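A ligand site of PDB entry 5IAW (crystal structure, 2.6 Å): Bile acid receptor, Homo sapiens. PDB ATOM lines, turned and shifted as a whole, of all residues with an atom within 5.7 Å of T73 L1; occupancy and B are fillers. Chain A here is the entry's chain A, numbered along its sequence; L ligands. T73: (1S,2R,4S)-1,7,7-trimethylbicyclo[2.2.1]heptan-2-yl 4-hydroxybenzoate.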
ATOM      1  N   PHE A  40     -17.837  -6.047 -11.327  1.00  0.00           N
ATOM      2  CA  PHE A  40     -17.391  -6.565 -10.083  1.00  0.00           C
ATOM      3  C   PHE A  40     -15.877  -6.386 -10.024  1.00  0.00           C
ATOM      4  O   PHE A  40     -15.306  -6.096  -8.965  1.00  0.00           O
ATOM      5  CB  PHE A  40     -17.793  -8.030  -9.943  1.00  0.00           C
ATOM      6  CG  PHE A  40     -17.178  -8.707  -8.764  1.00  0.00           C
ATOM      7  CD1 PHE A  40     -17.666  -8.495  -7.482  1.00  0.00           C
ATOM      8  CD2 PHE A  40     -16.084  -9.523  -8.928  1.00  0.00           C
ATOM      9  CE1 PHE A  40     -17.101  -9.118  -6.372  1.00  0.00           C
ATOM     10  CE2 PHE A  40     -15.494 -10.131  -7.824  1.00  0.00           C
ATOM     11  CZ  PHE A  40     -15.998  -9.937  -6.539  1.00  0.00           C
ATOM     12  N   LEU A  43     -15.212  -2.997  -8.991  1.00  0.00           N
ATOM     13  CA  LEU A  43     -15.417  -2.904  -7.553  1.00  0.00           C
ATOM     14  C   LEU A  43     -14.263  -3.466  -6.750  1.00  0.00           C
ATOM     15  O   LEU A  43     -13.941  -2.938  -5.675  1.00  0.00           O
ATOM     16  CB  LEU A  43     -16.691  -3.622  -7.153  1.00  0.00           C
ATOM     17  CG  LEU A  43     -17.973  -3.069  -7.808  1.00  0.00           C
ATOM     18  CD1 LEU A  43     -19.187  -3.860  -7.327  1.00  0.00           C
ATOM     19  CD2 LEU A  43     -18.230  -1.614  -7.509  1.00  0.00           C
ATOM     20  N   THR A  44     -13.636  -4.507  -7.271  1.00  0.00           N
ATOM     21  CA  THR A  44     -12.570  -5.158  -6.568  1.00  0.00           C
ATOM     22  C   THR A  44     -11.408  -4.220  -6.516  1.00  0.00           C
ATOM     23  O   THR A  44     -10.747  -4.101  -5.482  1.00  0.00           O
ATOM     24  CB  THR A  44     -12.231  -6.512  -7.170  1.00  0.00           C
ATOM     25  OG1 THR A  44     -13.283  -7.435  -6.891  1.00  0.00           O
ATOM     26  CG2 THR A  44     -10.992  -7.097  -6.575  1.00  0.00           C
ATOM     27  N   MET A  46     -11.748  -1.001  -6.533  1.00  0.00           N
ATOM     28  CA  MET A  46     -12.071   0.149  -5.695  1.00  0.00           C
ATOM     29  C   MET A  46     -11.916  -0.259  -4.247  1.00  0.00           C
ATOM     30  O   MET A  46     -11.408   0.473  -3.435  1.00  0.00           O
ATOM     31  CB  MET A  46     -13.481   0.629  -5.954  1.00  0.00           C
ATOM     32  CG  MET A  46     -13.683   1.231  -7.338  1.00  0.00           C
ATOM     33  SD  MET A  46     -15.349   2.009  -7.530  1.00  0.00           S
ATOM     34  CE  MET A  46     -16.294   0.551  -7.425  1.00  0.00           C
ATOM     35  N   ALA A  47     -12.347  -1.470  -3.956  1.00  0.00           N
ATOM     36  CA  ALA A  47     -12.216  -2.010  -2.609  1.00  0.00           C
ATOM     37  C   ALA A  47     -10.750  -2.100  -2.212  1.00  0.00           C
ATOM     38  O   ALA A  47     -10.376  -1.697  -1.125  1.00  0.00           O
ATOM     39  CB  ALA A  47     -12.905  -3.365  -2.503  1.00  0.00           C
ATOM     40  N   HIS A  50      -9.480   1.059  -1.264  1.00  0.00           N
ATOM     41  CA  HIS A  50      -9.920   1.553   0.015  1.00  0.00           C
ATOM     42  C   HIS A  50      -9.001   0.973   1.080  1.00  0.00           C
ATOM     43  O   HIS A  50      -8.525   1.682   1.951  1.00  0.00           O
ATOM     44  CB  HIS A  50     -11.382   1.166   0.294  1.00  0.00           C
ATOM     45  CG  HIS A  50     -12.414   2.036  -0.358  1.00  0.00           C
ATOM     46  ND1 HIS A  50     -12.770   3.279   0.143  1.00  0.00           N
ATOM     47  CD2 HIS A  50     -13.220   1.815  -1.424  1.00  0.00           C
ATOM     48  CE1 HIS A  50     -13.735   3.788  -0.613  1.00  0.00           C
ATOM     49  NE2 HIS A  50     -14.029   2.910  -1.565  1.00  0.00           N
ATOM     50  N   MET A  84     -14.324   2.521   5.128  1.00  0.00           N
ATOM     51  CA  MET A  84     -14.527   2.380   3.681  1.00  0.00           C
ATOM     52  C   MET A  84     -15.826   3.031   3.231  1.00  0.00           C
ATOM     53  O   MET A  84     -15.873   3.688   2.233  1.00  0.00           O
ATOM     54  CB  MET A  84     -14.539   0.915   3.291  1.00  0.00           C
ATOM     55  CG  MET A  84     -14.859   0.624   1.841  1.00  0.00           C
ATOM     56  SD  MET A  84     -14.972  -1.166   1.627  1.00  0.00           S
ATOM     57  CE  MET A  84     -13.235  -1.566   1.792  1.00  0.00           C
ATOM     58  N   PHE A  85     -16.881   2.879   4.034  1.00  0.00           N
ATOM     59  CA  PHE A  85     -18.134   3.547   3.732  1.00  0.00           C
ATOM     60  C   PHE A  85     -18.078   5.059   3.952  1.00  0.00           C
ATOM     61  O   PHE A  85     -18.693   5.843   3.239  1.00  0.00           O
ATOM     62  CB  PHE A  85     -19.291   2.835   4.426  1.00  0.00           C
ATOM     63  CG  PHE A  85     -19.789   1.596   3.677  1.00  0.00           C
ATOM     64  CD1 PHE A  85     -20.714   1.697   2.661  1.00  0.00           C
ATOM     65  CD2 PHE A  85     -19.292   0.364   3.940  1.00  0.00           C
ATOM     66  CE1 PHE A  85     -21.147   0.577   1.952  1.00  0.00           C
ATOM     67  CE2 PHE A  85     -19.701  -0.750   3.229  1.00  0.00           C
ATOM     68  CZ  PHE A  85     -20.636  -0.651   2.254  1.00  0.00           C
ATOM     69  N   SER A  88     -16.254   6.297   0.850  1.00  0.00           N
ATOM     70  CA  SER A  88     -17.214   6.221  -0.222  1.00  0.00           C
ATOM     71  C   SER A  88     -18.206   7.409  -0.181  1.00  0.00           C
ATOM     72  O   SER A  88     -18.388   8.064  -1.183  1.00  0.00           O
ATOM     73  CB  SER A  88     -17.926   4.884  -0.135  1.00  0.00           C
ATOM     74  OG  SER A  88     -16.937   3.943  -0.387  1.00  0.00           O
ATOM     75  N   ILE A 108     -24.733  -0.343  -9.523  1.00  0.00           N
ATOM     76  CA  ILE A 108     -24.474  -1.124  -8.310  1.00  0.00           C
ATOM     77  C   ILE A 108     -25.469  -2.259  -8.082  1.00  0.00           C
ATOM     78  O   ILE A 108     -25.111  -3.273  -7.473  1.00  0.00           O
ATOM     79  CB  ILE A 108     -24.496  -0.237  -7.068  1.00  0.00           C
ATOM     80  CG1 ILE A 108     -23.519   0.938  -7.196  1.00  0.00           C
ATOM     81  CG2 ILE A 108     -24.151  -1.046  -5.837  1.00  0.00           C
ATOM     82  CD1 ILE A 108     -22.060   0.542  -7.287  1.00  0.00           C
ATOM     83  N   ILE A 113     -24.982  -7.203  -5.973  1.00  0.00           N
ATOM     84  CA  ILE A 113     -25.450  -6.799  -4.657  1.00  0.00           C
ATOM     85  C   ILE A 113     -26.964  -6.696  -4.637  1.00  0.00           C
ATOM     86  O   ILE A 113     -27.579  -6.156  -5.562  1.00  0.00           O
ATOM     87  CB  ILE A 113     -24.878  -5.436  -4.286  1.00  0.00           C
ATOM     88  CG1 ILE A 113     -23.356  -5.466  -4.385  1.00  0.00           C
ATOM     89  CG2 ILE A 113     -25.300  -5.039  -2.896  1.00  0.00           C
ATOM     90  CD1 ILE A 113     -22.753  -4.088  -4.471  1.00  0.00           C
ATOM     91  N   MET A 121     -27.158   2.090   1.606  1.00  0.00           N
ATOM     92  CA  MET A 121     -25.858   2.672   1.187  1.00  0.00           C
ATOM     93  C   MET A 121     -26.008   4.101   0.681  1.00  0.00           C
ATOM     94  O   MET A 121     -25.375   5.019   1.171  1.00  0.00           O
ATOM     95  CB  MET A 121     -25.241   1.794   0.078  1.00  0.00           C
ATOM     96  CG  MET A 121     -23.779   1.997  -0.283  1.00  0.00           C
ATOM     97  SD  MET A 121     -23.165   0.724  -1.472  1.00  0.00           S
ATOM     98  CE  MET A 121     -23.884   1.447  -2.924  1.00  0.00           C
ATOM     99  N   TYR A 125     -25.109   7.873   2.016  1.00  0.00           N
ATOM    100  CA  TYR A 125     -24.404   8.849   1.179  1.00  0.00           C
ATOM    101  C   TYR A 125     -25.107  10.219   1.115  1.00  0.00           C
ATOM    102  O   TYR A 125     -24.446  11.267   1.153  1.00  0.00           O
ATOM    103  CB  TYR A 125     -24.194   8.324  -0.248  1.00  0.00           C
ATOM    104  CG  TYR A 125     -23.317   7.081  -0.376  1.00  0.00           C
ATOM    105  CD1 TYR A 125     -22.524   6.613   0.670  1.00  0.00           C
ATOM    106  CD2 TYR A 125     -23.266   6.382  -1.587  1.00  0.00           C
ATOM    107  CE1 TYR A 125     -21.727   5.486   0.524  1.00  0.00           C
ATOM    108  CE2 TYR A 125     -22.482   5.254  -1.739  1.00  0.00           C
ATOM    109  CZ  TYR A 125     -21.718   4.820  -0.680  1.00  0.00           C
ATOM    110  OH  TYR A 125     -20.924   3.713  -0.856  1.00  0.00           O
ATOM    111  N   HIS A 203     -22.118  -5.842   5.092  1.00  0.00           N
ATOM    112  CA  HIS A 203     -20.949  -6.095   4.297  1.00  0.00           C
ATOM    113  C   HIS A 203     -20.605  -7.553   4.310  1.00  0.00           C
ATOM    114  O   HIS A 203     -20.272  -8.093   3.276  1.00  0.00           O
ATOM    115  CB  HIS A 203     -19.737  -5.276   4.759  1.00  0.00           C
ATOM    116  CG  HIS A 203     -18.607  -5.317   3.782  1.00  0.00           C
ATOM    117  ND1 HIS A 203     -17.446  -6.016   4.012  1.00  0.00           N
ATOM    118  CD2 HIS A 203     -18.516  -4.813   2.531  1.00  0.00           C
ATOM    119  CE1 HIS A 203     -16.668  -5.926   2.954  1.00  0.00           C
ATOM    120  NE2 HIS A 203     -17.298  -5.202   2.036  1.00  0.00           N
ATOM    121  N   MET A 206     -22.957  -9.035   2.033  1.00  0.00           N
ATOM    122  CA  MET A 206     -22.613  -8.794   0.644  1.00  0.00           C
ATOM    123  C   MET A 206     -21.549  -9.778   0.207  1.00  0.00           C
ATOM    124  O   MET A 206     -21.612 -10.255  -0.907  1.00  0.00           O
ATOM    125  CB  MET A 206     -22.128  -7.370   0.398  1.00  0.00           C
ATOM    126  CG  MET A 206     -23.187  -6.288   0.570  1.00  0.00           C
ATOM    127  SD  MET A 206     -22.549  -4.573   0.643  1.00  0.00           S
ATOM    128  CE  MET A 206     -21.664  -4.657  -0.893  1.00  0.00           C
ATOM    129  N   LEU A 207     -20.597 -10.085   1.079  1.00  0.00           N
ATOM    130  CA  LEU A 207     -19.517 -11.023   0.769  1.00  0.00           C
ATOM    131  C   LEU A 207     -19.968 -12.447   0.764  1.00  0.00           C
ATOM    132  O   LEU A 207     -19.566 -13.222  -0.105  1.00  0.00           O
ATOM    133  CB  LEU A 207     -18.375 -10.979   1.789  1.00  0.00           C
ATOM    134  CG  LEU A 207     -17.580  -9.703   1.933  1.00  0.00           C
ATOM    135  CD1 LEU A 207     -16.416  -9.869   2.895  1.00  0.00           C
ATOM    136  CD2 LEU A 207     -17.088  -9.257   0.581  1.00  0.00           C
ATOM    137  N   TRP A 210     -21.890 -12.770  -2.512  1.00  0.00           N
ATOM    138  CA  TRP A 210     -20.980 -12.822  -3.660  1.00  0.00           C
ATOM    139  C   TRP A 210     -20.278 -14.177  -3.802  1.00  0.00           C
ATOM    140  O   TRP A 210     -20.103 -14.706  -4.916  1.00  0.00           O
ATOM    141  CB  TRP A 210     -19.910 -11.751  -3.522  1.00  0.00           C
ATOM    142  CG  TRP A 210     -20.243 -10.445  -4.117  1.00  0.00           C
ATOM    143  CD1 TRP A 210     -20.943 -10.205  -5.283  1.00  0.00           C
ATOM    144  CD2 TRP A 210     -19.820  -9.174  -3.638  1.00  0.00           C
ATOM    145  NE1 TRP A 210     -20.988  -8.865  -5.536  1.00  0.00           N
ATOM    146  CE2 TRP A 210     -20.298  -8.204  -4.549  1.00  0.00           C
ATOM    147  CE3 TRP A 210     -19.082  -8.751  -2.547  1.00  0.00           C
ATOM    148  CZ2 TRP A 210     -20.067  -6.830  -4.395  1.00  0.00           C
ATOM    149  CZ3 TRP A 210     -18.827  -7.371  -2.395  1.00  0.00           C
ATOM    150  CH2 TRP A 210     -19.320  -6.443  -3.306  1.00  0.00           C
ATOM    151  N   LYS A 216     -14.800 -14.411  -6.942  1.00  0.00           N
ATOM    152  CA  LYS A 216     -13.549 -14.628  -6.250  1.00  0.00           C
ATOM    153  C   LYS A 216     -13.014 -13.243  -5.846  1.00  0.00           C
ATOM    154  O   LYS A 216     -13.204 -12.276  -6.565  1.00  0.00           O
ATOM    155  CB  LYS A 216     -12.591 -15.385  -7.170  1.00  0.00           C
ATOM    156  CG  LYS A 216     -13.223 -16.618  -7.833  1.00  0.00           C
ATOM    157  CD  LYS A 216     -13.426 -17.777  -6.849  1.00  0.00           C
ATOM    158  CE  LYS A 216     -14.575 -18.703  -7.253  1.00  0.00           C
ATOM    159  NZ  LYS A 216     -14.678 -19.898  -6.362  1.00  0.00           N
ATOM    160  N   PHE A 217     -12.378 -13.145  -4.673  1.00  0.00           N
ATOM    161  CA  PHE A 217     -11.897 -11.832  -4.228  1.00  0.00           C
ATOM    162  C   PHE A 217     -10.379 -11.700  -4.553  1.00  0.00           C
ATOM    163  O   PHE A 217      -9.977 -11.988  -5.693  1.00  0.00           O
ATOM    164  CB  PHE A 217     -12.215 -11.597  -2.742  1.00  0.00           C
ATOM    165  CG  PHE A 217     -13.630 -11.878  -2.362  1.00  0.00           C
ATOM    166  CD1 PHE A 217     -14.677 -11.196  -2.945  1.00  0.00           C
ATOM    167  CD2 PHE A 217     -13.929 -12.839  -1.397  1.00  0.00           C
ATOM    168  CE1 PHE A 217     -15.976 -11.440  -2.589  1.00  0.00           C
ATOM    169  CE2 PHE A 217     -15.242 -13.092  -1.042  1.00  0.00           C
ATOM    170  CZ  PHE A 217     -16.258 -12.392  -1.647  1.00  0.00           C
ATOM    171  N   THR A 218      -9.585 -11.187  -3.606  1.00  0.00           N
ATOM    172  CA  THR A 218      -8.134 -11.146  -3.722  1.00  0.00           C
ATOM    173  C   THR A 218      -7.601 -11.580  -2.340  1.00  0.00           C
ATOM    174  O   THR A 218      -8.341 -11.542  -1.327  1.00  0.00           O
ATOM    175  CB  THR A 218      -7.571  -9.748  -4.066  1.00  0.00           C
ATOM    176  OG1 THR A 218      -7.783  -8.811  -2.999  1.00  0.00           O
ATOM    177  CG2 THR A 218      -8.219  -9.177  -5.269  1.00  0.00           C
ATOM    178  N   LEU A 221      -8.052  -8.725   0.403  1.00  0.00           N
ATOM    179  CA  LEU A 221      -9.434  -8.559   0.770  1.00  0.00           C
ATOM    180  C   LEU A 221      -9.861  -9.698   1.666  1.00  0.00           C
ATOM    181  O   LEU A 221     -10.581  -9.473   2.655  1.00  0.00           O
ATOM    182  CB  LEU A 221     -10.296  -8.426  -0.442  1.00  0.00           C
ATOM    183  CG  LEU A 221      -9.901  -7.237  -1.318  1.00  0.00           C
ATOM    184  CD1 LEU A 221     -11.007  -6.996  -2.314  1.00  0.00           C
ATOM    185  CD2 LEU A 221      -9.633  -5.973  -0.551  1.00  0.00           C
ATOM    186  N   TRP A 225     -10.948  -9.137   5.984  1.00  0.00           N
ATOM    187  CA  TRP A 225     -12.253  -9.558   6.459  1.00  0.00           C
ATOM    188  C   TRP A 225     -12.380 -11.007   6.731  1.00  0.00           C
ATOM    189  O   TRP A 225     -13.484 -11.473   6.656  1.00  0.00           O
ATOM    190  CB  TRP A 225     -13.309  -9.197   5.428  1.00  0.00           C
ATOM    191  CG  TRP A 225     -13.423  -7.730   5.302  1.00  0.00           C
ATOM    192  CD1 TRP A 225     -13.697  -6.838   6.299  1.00  0.00           C
ATOM    193  CD2 TRP A 225     -13.290  -6.985   4.101  1.00  0.00           C
ATOM    194  NE1 TRP A 225     -13.721  -5.573   5.771  1.00  0.00           N
ATOM    195  CE2 TRP A 225     -13.477  -5.643   4.422  1.00  0.00           C
ATOM    196  CE3 TRP A 225     -13.059  -7.338   2.762  1.00  0.00           C
ATOM    197  CZ2 TRP A 225     -13.406  -4.648   3.472  1.00  0.00           C
ATOM    198  CZ3 TRP A 225     -12.988  -6.344   1.812  1.00  0.00           C
ATOM    199  CH2 TRP A 225     -13.144  -5.021   2.173  1.00  0.00           C
HETATM  200  O1  T73 L   1     -16.479  -4.794  -0.212  1.00  0.00           O
HETATM  201  C8  T73 L   1     -16.234  -4.502  -1.361  1.00  0.00           C
HETATM  202  O   T73 L   1     -16.344  -3.060  -1.516  1.00  0.00           O
HETATM  203  C6  T73 L   1     -17.167  -2.249  -2.340  1.00  0.00           C
HETATM  204  C7  T73 L   1     -16.451  -0.929  -2.775  1.00  0.00           C
HETATM  205  C2  T73 L   1     -17.540   0.149  -2.621  1.00  0.00           C
HETATM  206  C5  T73 L   1     -18.364  -1.613  -1.668  1.00  0.00           C
HETATM  207  C15 T73 L   1     -19.414  -2.585  -1.278  1.00  0.00           C
HETATM  208  C4  T73 L   1     -18.058  -0.637  -0.525  1.00  0.00           C
HETATM  209  C3  T73 L   1     -17.650   0.678  -1.197  1.00  0.00           C
HETATM  210  C1  T73 L   1     -18.772  -0.671  -2.732  1.00  0.00           C
HETATM  211  C16 T73 L   1     -19.987   0.175  -2.404  1.00  0.00           C
HETATM  212  C   T73 L   1     -18.883  -1.291  -4.096  1.00  0.00           C
HETATM  213  C9  T73 L   1     -15.655  -5.538  -2.273  1.00  0.00           C
HETATM  214  C14 T73 L   1     -15.081  -6.680  -1.718  1.00  0.00           C
HETATM  215  C13 T73 L   1     -14.463  -7.664  -2.504  1.00  0.00           C
HETATM  216  C12 T73 L   1     -14.455  -7.485  -3.907  1.00  0.00           C
HETATM  217  O2  T73 L   1     -13.854  -8.416  -4.729  1.00  0.00           O
HETATM  218  C11 T73 L   1     -15.027  -6.335  -4.466  1.00  0.00           C
HETATM  219  C10 T73 L   1     -15.599  -5.385  -3.642  1.00  0.00           C
HETATM  220  O1  T73 L   2     -15.459   3.285  -3.915  1.00  0.00           O
HETATM  221  C8  T73 L   2     -15.261   4.115  -4.792  1.00  0.00           C
HETATM  222  O   T73 L   2     -16.396   4.802  -5.346  1.00  0.00           O
HETATM  223  C6  T73 L   2     -17.660   4.180  -5.165  1.00  0.00           C
HETATM  224  C7  T73 L   2     -18.183   3.734  -6.540  1.00  0.00           C
HETATM  225  C2  T73 L   2     -19.350   4.642  -6.635  1.00  0.00           C
HETATM  226  C5  T73 L   2     -18.755   5.084  -4.647  1.00  0.00           C
HETATM  227  C15 T73 L   2     -18.668   5.080  -3.171  1.00  0.00           C
HETATM  228  C4  T73 L   2     -18.641   6.482  -5.222  1.00  0.00           C
HETATM  229  C3  T73 L   2     -18.769   6.084  -6.688  1.00  0.00           C
HETATM  230  C1  T73 L   2     -20.010   4.548  -5.304  1.00  0.00           C
HETATM  231  C16 T73 L   2     -21.215   5.464  -5.326  1.00  0.00           C
HETATM  232  C   T73 L   2     -20.441   3.135  -4.947  1.00  0.00           C
HETATM  233  C9  T73 L   2     -13.898   4.526  -5.221  1.00  0.00           C
HETATM  234  C14 T73 L   2     -12.764   4.337  -4.413  1.00  0.00           C
HETATM  235  C13 T73 L   2     -11.477   4.764  -4.787  1.00  0.00           C
HETATM  236  C12 T73 L   2     -11.390   5.368  -6.017  1.00  0.00           C
HETATM  237  O2  T73 L   2     -10.211   5.826  -6.505  1.00  0.00           O
HETATM  238  C11 T73 L   2     -12.501   5.563  -6.827  1.00  0.00           C
HETATM  239  C10 T73 L   2     -13.747   5.146  -6.441  1.00  0.00           C
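A ring nitrogen (NE2) of His 203 is in hydrogen-bond range of an oxygen (O1) of T73 L1 (2.4 Å). The side-chain hydroxyl (OG1) of Thr 44 lies within hydrogen-bond range of an oxygen (O2) of T73 L1. A ring nitrogen (NE2) of His 50 lies within hydrogen-bond range of an oxygen (O1) of T73 L2 (2.8 Å).
OG1 of Thr 44 sits at hydrogen-bond distance from O of Phe 40. The side-chain sulfur of Met 121 lies close to the side-chain hydroxyl of Tyr 125. OG of Ser 88 lies within hydrogen-bond range of O of Met 84 (2.8 Å). A ring nitrogen (NE2) of His 50 lies close to the side-chain hydroxyl (OG) of Ser 88 (3.3 Å). N of Leu 221 lies close to OG1 of Thr 218.
Residues that only touch T73 L1: Met 206 (3.1 Å), Phe 40 (3.2 Å), Met 121 (3.4 Å), Phe 217 (3.4 Å), Ser 88 (3.4 Å), Leu 43 (3.5 Å), Ala 47 (3.5 Å), Leu 221 (3.5 Å), Trp 210 (3.7 Å), Phe 85 (3.8 Å), Met 84 (3.8 Å), Tyr 125 (3.97 Å) and Leu 207 (3.99 Å). Hydrophobic or aromatic side chains that line T73 L1: Phe 40, Leu 43, Ala 47, Met 84, Phe 85, Met 121, His 203, Met 206, Leu 207, Trp 210, Phe 217 and Leu 221.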
